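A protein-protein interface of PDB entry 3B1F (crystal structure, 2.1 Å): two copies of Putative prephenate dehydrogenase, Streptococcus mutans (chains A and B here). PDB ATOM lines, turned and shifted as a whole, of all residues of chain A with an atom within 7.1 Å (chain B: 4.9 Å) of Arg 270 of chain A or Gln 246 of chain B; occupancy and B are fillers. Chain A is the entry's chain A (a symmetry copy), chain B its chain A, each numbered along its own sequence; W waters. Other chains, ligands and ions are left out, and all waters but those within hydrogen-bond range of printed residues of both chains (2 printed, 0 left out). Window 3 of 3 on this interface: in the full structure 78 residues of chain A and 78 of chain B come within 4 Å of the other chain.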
ATOM      1  N   SER A 264     -24.099  -6.244 -13.370  1.00  0.00           N
ATOM      2  CA  SER A 264     -25.222  -7.148 -13.599  1.00  0.00           C
ATOM      3  C   SER A 264     -24.864  -8.305 -14.542  1.00  0.00           C
ATOM      4  O   SER A 264     -25.180  -9.456 -14.264  1.00  0.00           O
ATOM      5  CB  SER A 264     -26.418  -6.369 -14.146  1.00  0.00           C
ATOM      6  OG  SER A 264     -27.441  -7.243 -14.571  1.00  0.00           O
ATOM      7  N   ASN A 265     -24.168  -7.998 -15.631  1.00  0.00           N
ATOM      8  CA  ASN A 265     -23.587  -9.045 -16.520  1.00  0.00           C
ATOM      9  C   ASN A 265     -22.691 -10.008 -15.823  1.00  0.00           C
ATOM     10  O   ASN A 265     -22.782 -11.229 -16.073  1.00  0.00           O
ATOM     11  CB  ASN A 265     -22.856  -8.480 -17.725  1.00  0.00           C
ATOM     12  CG  ASN A 265     -23.816  -7.699 -18.657  1.00  0.00           C
ATOM     13  OD1 ASN A 265     -25.087  -7.808 -18.561  1.00  0.00           O
ATOM     14  ND2 ASN A 265     -23.232  -6.889 -19.531  1.00  0.00           N
ATOM     15  N   LEU A 266     -21.849  -9.508 -14.916  1.00  0.00           N
ATOM     16  CA  LEU A 266     -20.981 -10.466 -14.193  1.00  0.00           C
ATOM     17  C   LEU A 266     -21.775 -11.442 -13.327  1.00  0.00           C
ATOM     18  O   LEU A 266     -21.476 -12.645 -13.319  1.00  0.00           O
ATOM     19  CB  LEU A 266     -19.913  -9.760 -13.349  1.00  0.00           C
ATOM     20  CG  LEU A 266     -18.967  -8.829 -14.071  1.00  0.00           C
ATOM     21  CD1 LEU A 266     -18.175  -8.117 -12.983  1.00  0.00           C
ATOM     22  CD2 LEU A 266     -18.003  -9.526 -15.121  1.00  0.00           C
ATOM     23  N   ILE A 267     -22.791 -10.937 -12.608  1.00  0.00           N
ATOM     24  CA  ILE A 267     -23.635 -11.764 -11.788  1.00  0.00           C
ATOM     25  C   ILE A 267     -24.362 -12.817 -12.659  1.00  0.00           C
ATOM     26  O   ILE A 267     -24.395 -14.010 -12.341  1.00  0.00           O
ATOM     27  CB  ILE A 267     -24.673 -10.846 -10.959  1.00  0.00           C
ATOM     28  CG1 ILE A 267     -23.901  -9.964  -9.920  1.00  0.00           C
ATOM     29  CG2 ILE A 267     -25.716 -11.704 -10.263  1.00  0.00           C
ATOM     30  CD1 ILE A 267     -24.745  -8.765  -9.365  1.00  0.00           C
ATOM     31  N   LYS A 268     -24.923 -12.386 -13.775  1.00  0.00           N
ATOM     32  CA  LYS A 268     -25.675 -13.314 -14.672  1.00  0.00           C
ATOM     33  C   LYS A 268     -24.728 -14.374 -15.169  1.00  0.00           C
ATOM     34  O   LYS A 268     -25.074 -15.546 -15.183  1.00  0.00           O
ATOM     35  CB  LYS A 268     -26.306 -12.562 -15.852  1.00  0.00           C
ATOM     36  CG  LYS A 268     -27.603 -11.807 -15.419  1.00  0.00           C
ATOM     37  CD  LYS A 268     -27.947 -10.742 -16.489  1.00  0.00           C
ATOM     38  CE  LYS A 268     -29.322 -10.234 -16.282  1.00  0.00           C
ATOM     39  NZ  LYS A 268     -29.512  -9.229 -17.369  1.00  0.00           N
ATOM     40  N   ALA A 269     -23.507 -13.989 -15.531  1.00  0.00           N
ATOM     41  CA  ALA A 269     -22.537 -15.012 -15.964  1.00  0.00           C
ATOM     42  C   ALA A 269     -21.989 -15.881 -14.795  1.00  0.00           C
ATOM     43  O   ALA A 269     -21.226 -16.799 -15.032  1.00  0.00           O
ATOM     44  CB  ALA A 269     -21.426 -14.358 -16.725  1.00  0.00           C
ATOM     45  N   ARG A 270     -22.359 -15.598 -13.524  1.00  0.00           N
ATOM     46  CA  ARG A 270     -21.703 -16.283 -12.360  1.00  0.00           C
ATOM     47  C   ARG A 270     -20.180 -16.227 -12.493  1.00  0.00           C
ATOM     48  O   ARG A 270     -19.463 -17.203 -12.223  1.00  0.00           O
ATOM     49  CB  ARG A 270     -22.170 -17.753 -12.187  1.00  0.00           C
ATOM     50  CG  ARG A 270     -23.704 -17.992 -12.315  1.00  0.00           C
ATOM     51  CD  ARG A 270     -24.095 -19.473 -11.954  1.00  0.00           C
ATOM     52  NE  ARG A 270     -23.063 -20.031 -11.040  1.00  0.00           N
ATOM     53  CZ  ARG A 270     -23.171 -20.144  -9.700  1.00  0.00           C
ATOM     54  NH1 ARG A 270     -24.292 -19.787  -9.067  1.00  0.00           N
ATOM     55  NH2 ARG A 270     -22.142 -20.604  -8.981  1.00  0.00           N
ATOM     56  N   ASP A 271     -19.671 -15.069 -12.898  1.00  0.00           N
ATOM     57  CA  ASP A 271     -18.231 -14.939 -13.105  1.00  0.00           C
ATOM     58  C   ASP A 271     -17.547 -14.581 -11.782  1.00  0.00           C
ATOM     59  O   ASP A 271     -17.317 -13.416 -11.494  1.00  0.00           O
ATOM     60  CB  ASP A 271     -18.014 -13.813 -14.067  1.00  0.00           C
ATOM     61  CG  ASP A 271     -16.585 -13.698 -14.516  1.00  0.00           C
ATOM     62  OD1 ASP A 271     -15.626 -14.179 -13.835  1.00  0.00           O
ATOM     63  OD2 ASP A 271     -16.435 -13.056 -15.559  1.00  0.00           O
ATOM     64  N   GLU A 272     -17.144 -15.597 -11.048  1.00  0.00           N
ATOM     65  CA  GLU A 272     -16.700 -15.426  -9.712  1.00  0.00           C
ATOM     66  C   GLU A 272     -15.379 -14.628  -9.652  1.00  0.00           C
ATOM     67  O   GLU A 272     -15.207 -13.755  -8.833  1.00  0.00           O
ATOM     68  CB  GLU A 272     -16.547 -16.819  -9.118  1.00  0.00           C
ATOM     69  CG  GLU A 272     -15.872 -16.801  -7.854  1.00  0.00           C
ATOM     70  CD  GLU A 272     -15.605 -18.216  -7.334  1.00  0.00           C
ATOM     71  OE1 GLU A 272     -16.486 -19.110  -7.482  1.00  0.00           O
ATOM     72  OE2 GLU A 272     -14.495 -18.409  -6.797  1.00  0.00           O
ATOM     73  N   ASN A 273     -14.426 -14.969 -10.507  1.00  0.00           N
ATOM     74  CA  ASN A 273     -13.143 -14.246 -10.528  1.00  0.00           C
ATOM     75  C   ASN A 273     -13.283 -12.754 -10.869  1.00  0.00           C
ATOM     76  O   ASN A 273     -12.593 -11.920 -10.292  1.00  0.00           O
ATOM     77  CB  ASN A 273     -12.245 -14.895 -11.534  1.00  0.00           C
ATOM     78  CG  ASN A 273     -11.886 -16.273 -11.153  1.00  0.00           C
ATOM     79  OD1 ASN A 273     -11.175 -16.470 -10.184  1.00  0.00           O
ATOM     80  ND2 ASN A 273     -12.292 -17.244 -11.954  1.00  0.00           N
ATOM     81  N   ILE A 275     -16.016 -10.975 -10.406  1.00  0.00           N
ATOM     82  CA  ILE A 275     -16.786 -10.295  -9.373  1.00  0.00           C
ATOM     83  C   ILE A 275     -15.840 -10.008  -8.192  1.00  0.00           C
ATOM     84  O   ILE A 275     -15.854  -8.920  -7.635  1.00  0.00           O
ATOM     85  CB  ILE A 275     -17.979 -11.098  -8.908  1.00  0.00           C
ATOM     86  CG1 ILE A 275     -19.112 -11.036  -9.932  1.00  0.00           C
ATOM     87  CG2 ILE A 275     -18.456 -10.532  -7.535  1.00  0.00           C
ATOM     88  CD1 ILE A 275     -19.986 -12.169  -9.787  1.00  0.00           C
ATOM     89  N   LYS B  77     -19.496 -21.406   0.219  1.00  0.00           N
ATOM     90  CA  LYS B  77     -19.292 -22.611  -0.617  1.00  0.00           C
ATOM     91  C   LYS B  77     -18.753 -23.747   0.160  1.00  0.00           C
ATOM     92  O   LYS B  77     -19.063 -24.896  -0.128  1.00  0.00           O
ATOM     93  CB  LYS B  77     -18.364 -22.388  -1.838  1.00  0.00           C
ATOM     94  CG  LYS B  77     -18.743 -21.223  -2.745  1.00  0.00           C
ATOM     95  CD  LYS B  77     -19.870 -21.546  -3.748  1.00  0.00           C
ATOM     96  CE  LYS B  77     -20.921 -20.383  -3.794  1.00  0.00           C
ATOM     97  NZ  LYS B  77     -21.726 -20.482  -5.022  1.00  0.00           N
ATOM     98  N   LEU B 242     -23.093 -12.391  -3.547  1.00  0.00           N
ATOM     99  CA  LEU B 242     -23.711 -12.105  -4.834  1.00  0.00           C
ATOM    100  C   LEU B 242     -24.078 -13.351  -5.633  1.00  0.00           C
ATOM    101  O   LEU B 242     -25.163 -13.438  -6.155  1.00  0.00           O
ATOM    102  CB  LEU B 242     -22.793 -11.246  -5.695  1.00  0.00           C
ATOM    103  CG  LEU B 242     -23.033  -9.757  -5.592  1.00  0.00           C
ATOM    104  CD1 LEU B 242     -23.052  -9.211  -4.132  1.00  0.00           C
ATOM    105  CD2 LEU B 242     -22.046  -8.939  -6.552  1.00  0.00           C
ATOM    106  N   LEU B 243     -23.163 -14.308  -5.712  1.00  0.00           N
ATOM    107  CA  LEU B 243     -23.413 -15.539  -6.446  1.00  0.00           C
ATOM    108  C   LEU B 243     -24.455 -16.493  -5.808  1.00  0.00           C
ATOM    109  O   LEU B 243     -24.939 -17.428  -6.464  1.00  0.00           O
ATOM    110  CB  LEU B 243     -22.060 -16.278  -6.642  1.00  0.00           C
ATOM    111  CG  LEU B 243     -21.084 -15.541  -7.624  1.00  0.00           C
ATOM    112  CD1 LEU B 243     -19.864 -16.339  -7.848  1.00  0.00           C
ATOM    113  CD2 LEU B 243     -21.668 -15.240  -8.998  1.00  0.00           C
ATOM    114  N   THR B 244     -24.746 -16.302  -4.523  1.00  0.00           N
ATOM    115  CA  THR B 244     -25.813 -17.054  -3.898  1.00  0.00           C
ATOM    116  C   THR B 244     -27.082 -16.198  -3.663  1.00  0.00           C
ATOM    117  O   THR B 244     -28.067 -16.703  -3.115  1.00  0.00           O
ATOM    118  CB  THR B 244     -25.373 -17.709  -2.531  1.00  0.00           C
ATOM    119  OG1 THR B 244     -25.016 -16.654  -1.630  1.00  0.00           O
ATOM    120  CG2 THR B 244     -24.161 -18.639  -2.751  1.00  0.00           C
ATOM    121  N   ASN B 245     -27.110 -14.952  -4.139  1.00  0.00           N
ATOM    122  CA  ASN B 245     -28.324 -14.124  -3.999  1.00  0.00           C
ATOM    123  C   ASN B 245     -28.596 -13.366  -5.326  1.00  0.00           C
ATOM    124  O   ASN B 245     -28.936 -12.143  -5.320  1.00  0.00           O
ATOM    125  CB  ASN B 245     -28.158 -13.104  -2.832  1.00  0.00           C
ATOM    126  CG  ASN B 245     -29.505 -12.640  -2.255  1.00  0.00           C
ATOM    127  OD1 ASN B 245     -30.527 -13.311  -2.465  1.00  0.00           O
ATOM    128  ND2 ASN B 245     -29.504 -11.542  -1.498  1.00  0.00           N
ATOM    129  N   GLN B 246     -28.447 -14.074  -6.438  1.00  0.00           N
ATOM    130  CA  GLN B 246     -28.410 -13.430  -7.777  1.00  0.00           C
ATOM    131  C   GLN B 246     -29.699 -12.688  -8.140  1.00  0.00           C
ATOM    132  O   GLN B 246     -29.653 -11.517  -8.515  1.00  0.00           O
ATOM    133  CB  GLN B 246     -28.109 -14.444  -8.882  1.00  0.00           C
ATOM    134  CG  GLN B 246     -26.676 -15.006  -8.865  1.00  0.00           C
ATOM    135  CD  GLN B 246     -26.614 -16.182  -9.796  1.00  0.00           C
ATOM    136  OE1 GLN B 246     -27.087 -17.236  -9.433  1.00  0.00           O
ATOM    137  NE2 GLN B 246     -26.181 -15.977 -11.038  1.00  0.00           N
ATOM    138  N   GLU B 247     -30.822 -13.409  -8.063  1.00  0.00           N
ATOM    139  CA  GLU B 247     -32.132 -12.872  -8.386  1.00  0.00           C
ATOM    140  C   GLU B 247     -32.564 -11.569  -7.646  1.00  0.00           C
ATOM    141  O   GLU B 247     -33.039 -10.578  -8.267  1.00  0.00           O
ATOM    142  CB  GLU B 247     -33.218 -13.943  -8.080  1.00  0.00           C
ATOM    143  CG  GLU B 247     -34.526 -13.526  -8.685  1.00  0.00           C
ATOM    144  CD  GLU B 247     -35.641 -14.544  -8.423  1.00  0.00           C
ATOM    145  OE1 GLU B 247     -35.655 -15.227  -7.417  1.00  0.00           O
ATOM    146  OE2 GLU B 247     -36.538 -14.615  -9.204  1.00  0.00           O
ATOM    147  N   ALA B 248     -32.509 -11.616  -6.326  1.00  0.00           N
ATOM    148  CA  ALA B 248     -32.782 -10.415  -5.566  1.00  0.00           C
ATOM    149  C   ALA B 248     -31.839  -9.231  -5.938  1.00  0.00           C
ATOM    150  O   ALA B 248     -32.264  -8.064  -6.092  1.00  0.00           O
ATOM    151  CB  ALA B 248     -32.702 -10.742  -4.056  1.00  0.00           C
ATOM    152  N   VAL B 249     -30.550  -9.482  -5.938  1.00  0.00           N
ATOM    153  CA  VAL B 249     -29.576  -8.418  -6.260  1.00  0.00           C
ATOM    154  C   VAL B 249     -29.763  -7.863  -7.697  1.00  0.00           C
ATOM    155  O   VAL B 249     -29.848  -6.625  -7.903  1.00  0.00           O
ATOM    156  CB  VAL B 249     -28.152  -8.885  -5.971  1.00  0.00           C
ATOM    157  CG1 VAL B 249     -27.215  -7.981  -6.571  1.00  0.00           C
ATOM    158  CG2 VAL B 249     -27.879  -8.863  -4.355  1.00  0.00           C
ATOM    159  N   LEU B 250     -29.924  -8.738  -8.671  1.00  0.00           N
ATOM    160  CA  LEU B 250     -30.223  -8.275 -10.028  1.00  0.00           C
ATOM    161  C   LEU B 250     -31.520  -7.449 -10.078  1.00  0.00           C
ATOM    162  O   LEU B 250     -31.618  -6.503 -10.829  1.00  0.00           O
ATOM    163  CB  LEU B 250     -30.267  -9.433 -11.076  1.00  0.00           C
ATOM    164  CG  LEU B 250     -28.979 -10.212 -11.331  1.00  0.00           C
ATOM    165  CD1 LEU B 250     -29.278 -11.600 -12.060  1.00  0.00           C
ATOM    166  CD2 LEU B 250     -28.000  -9.253 -12.129  1.00  0.00           C
ATOM    167  N   ASP B 251     -32.520  -7.836  -9.297  1.00  0.00           N
ATOM    168  CA  ASP B 251     -33.780  -7.122  -9.286  1.00  0.00           C
ATOM    169  C   ASP B 251     -33.575  -5.703  -8.717  1.00  0.00           C
ATOM    170  O   ASP B 251     -34.059  -4.756  -9.291  1.00  0.00           O
ATOM    171  CB  ASP B 251     -34.872  -7.905  -8.525  1.00  0.00           C
ATOM    172  CG  ASP B 251     -36.098  -7.043  -8.281  1.00  0.00           C
ATOM    173  OD1 ASP B 251     -36.877  -6.840  -9.183  1.00  0.00           O
ATOM    174  OD2 ASP B 251     -36.223  -6.430  -7.228  1.00  0.00           O
HETATM  175  O   HOH W   1     -25.289 -19.977  -6.531  1.00  0.00           O
HETATM  176  O   HOH W   2     -30.015  -6.164 -12.745  1.00  0.00           O
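No position is printed for both chains.
Of the 11 pairs that touch across the chains among the printed residues, none has its exchanged pair printed and touching as well.
Among the printed residues, merely in contact across the chains: Ser 264 of chain A with Leu 250 of chain B (3.2 Å), Ile 267 of chain A with Leu 242 of chain B (3.9 Å), Ile 267 of chain A with Val 249 of chain B (3.8 Å), Ile 267 of chain A with Leu 250 of chain B (3.7 Å), Lys 268 of chain A with Leu 250 of chain B (3.8 Å), Arg 270 of chain A with Lys 77 of chain B (3.98 Å), Arg 270 of chain A with Leu 243 of chain B (3.5 Å), Arg 270 of chain A with Gln 246 of chain B (3.4 Å), Glu 272 of chain A with Leu 243 of chain B (3.6 Å) and Ile 275 of chain A with Leu 243 of chain B (3.6 Å).
Water W2 bridges O of Leu 250 of chain B (2.5 Å) and OG of Ser 264 of chain A (3.3 Å).
Water W1 lies within hydrogen-bond range of O of Leu 243 of chain B (2.6 Å) and NH1 of Arg 270 of chain A (2.7 Å).
NE2 of Gln 246 of chain B is in hydrogen-bond range of O of Ile 267 of chain A (3.0 Å).
Printed residues of chain B within 4 Å of Ser 264 of chain A: Leu 250.
Printed residues of chain B within 4 Å of Ile 267 of chain A: Leu 242, Gln 246, Val 249 and Leu 250.
Of the printed residues of chain B, Arg 270 of chain A touches Lys 77, Leu 243 and Gln 246.
Printed residues of chain A within 4 Å of Leu 243 of chain B: Arg 270 (3.5 Å), Glu 272 (3.6 Å) and Ile 275 (3.6 Å).
Gln 246 of chain B touches just these residues of chain A: Ile 267 (3.0 Å) and Arg 270 (3.4 Å).
Of the printed residues of chain A, Leu 250 of chain B touches Ser 264, Ile 267 and Lys 268.
The nearest printed residue of chain A that does not touch Leu 243 of chain B is Asp 271 of chain A (4.4 Å).
Of the 11 printed residues of chain B, 6 touch a printed residue of chain A.
Printed residues of chain B that touch a printed residue of chain A: Lys 77, Leu 242, Leu 243, Gln 246, Val 249 and Leu 250.
Hydrophobic or aromatic side chains of chain B that line the printed part of chain A: Leu 242, Leu 243, Val 249 and Leu 250.
Among the printed residues, 11 pairs touch across the chains.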
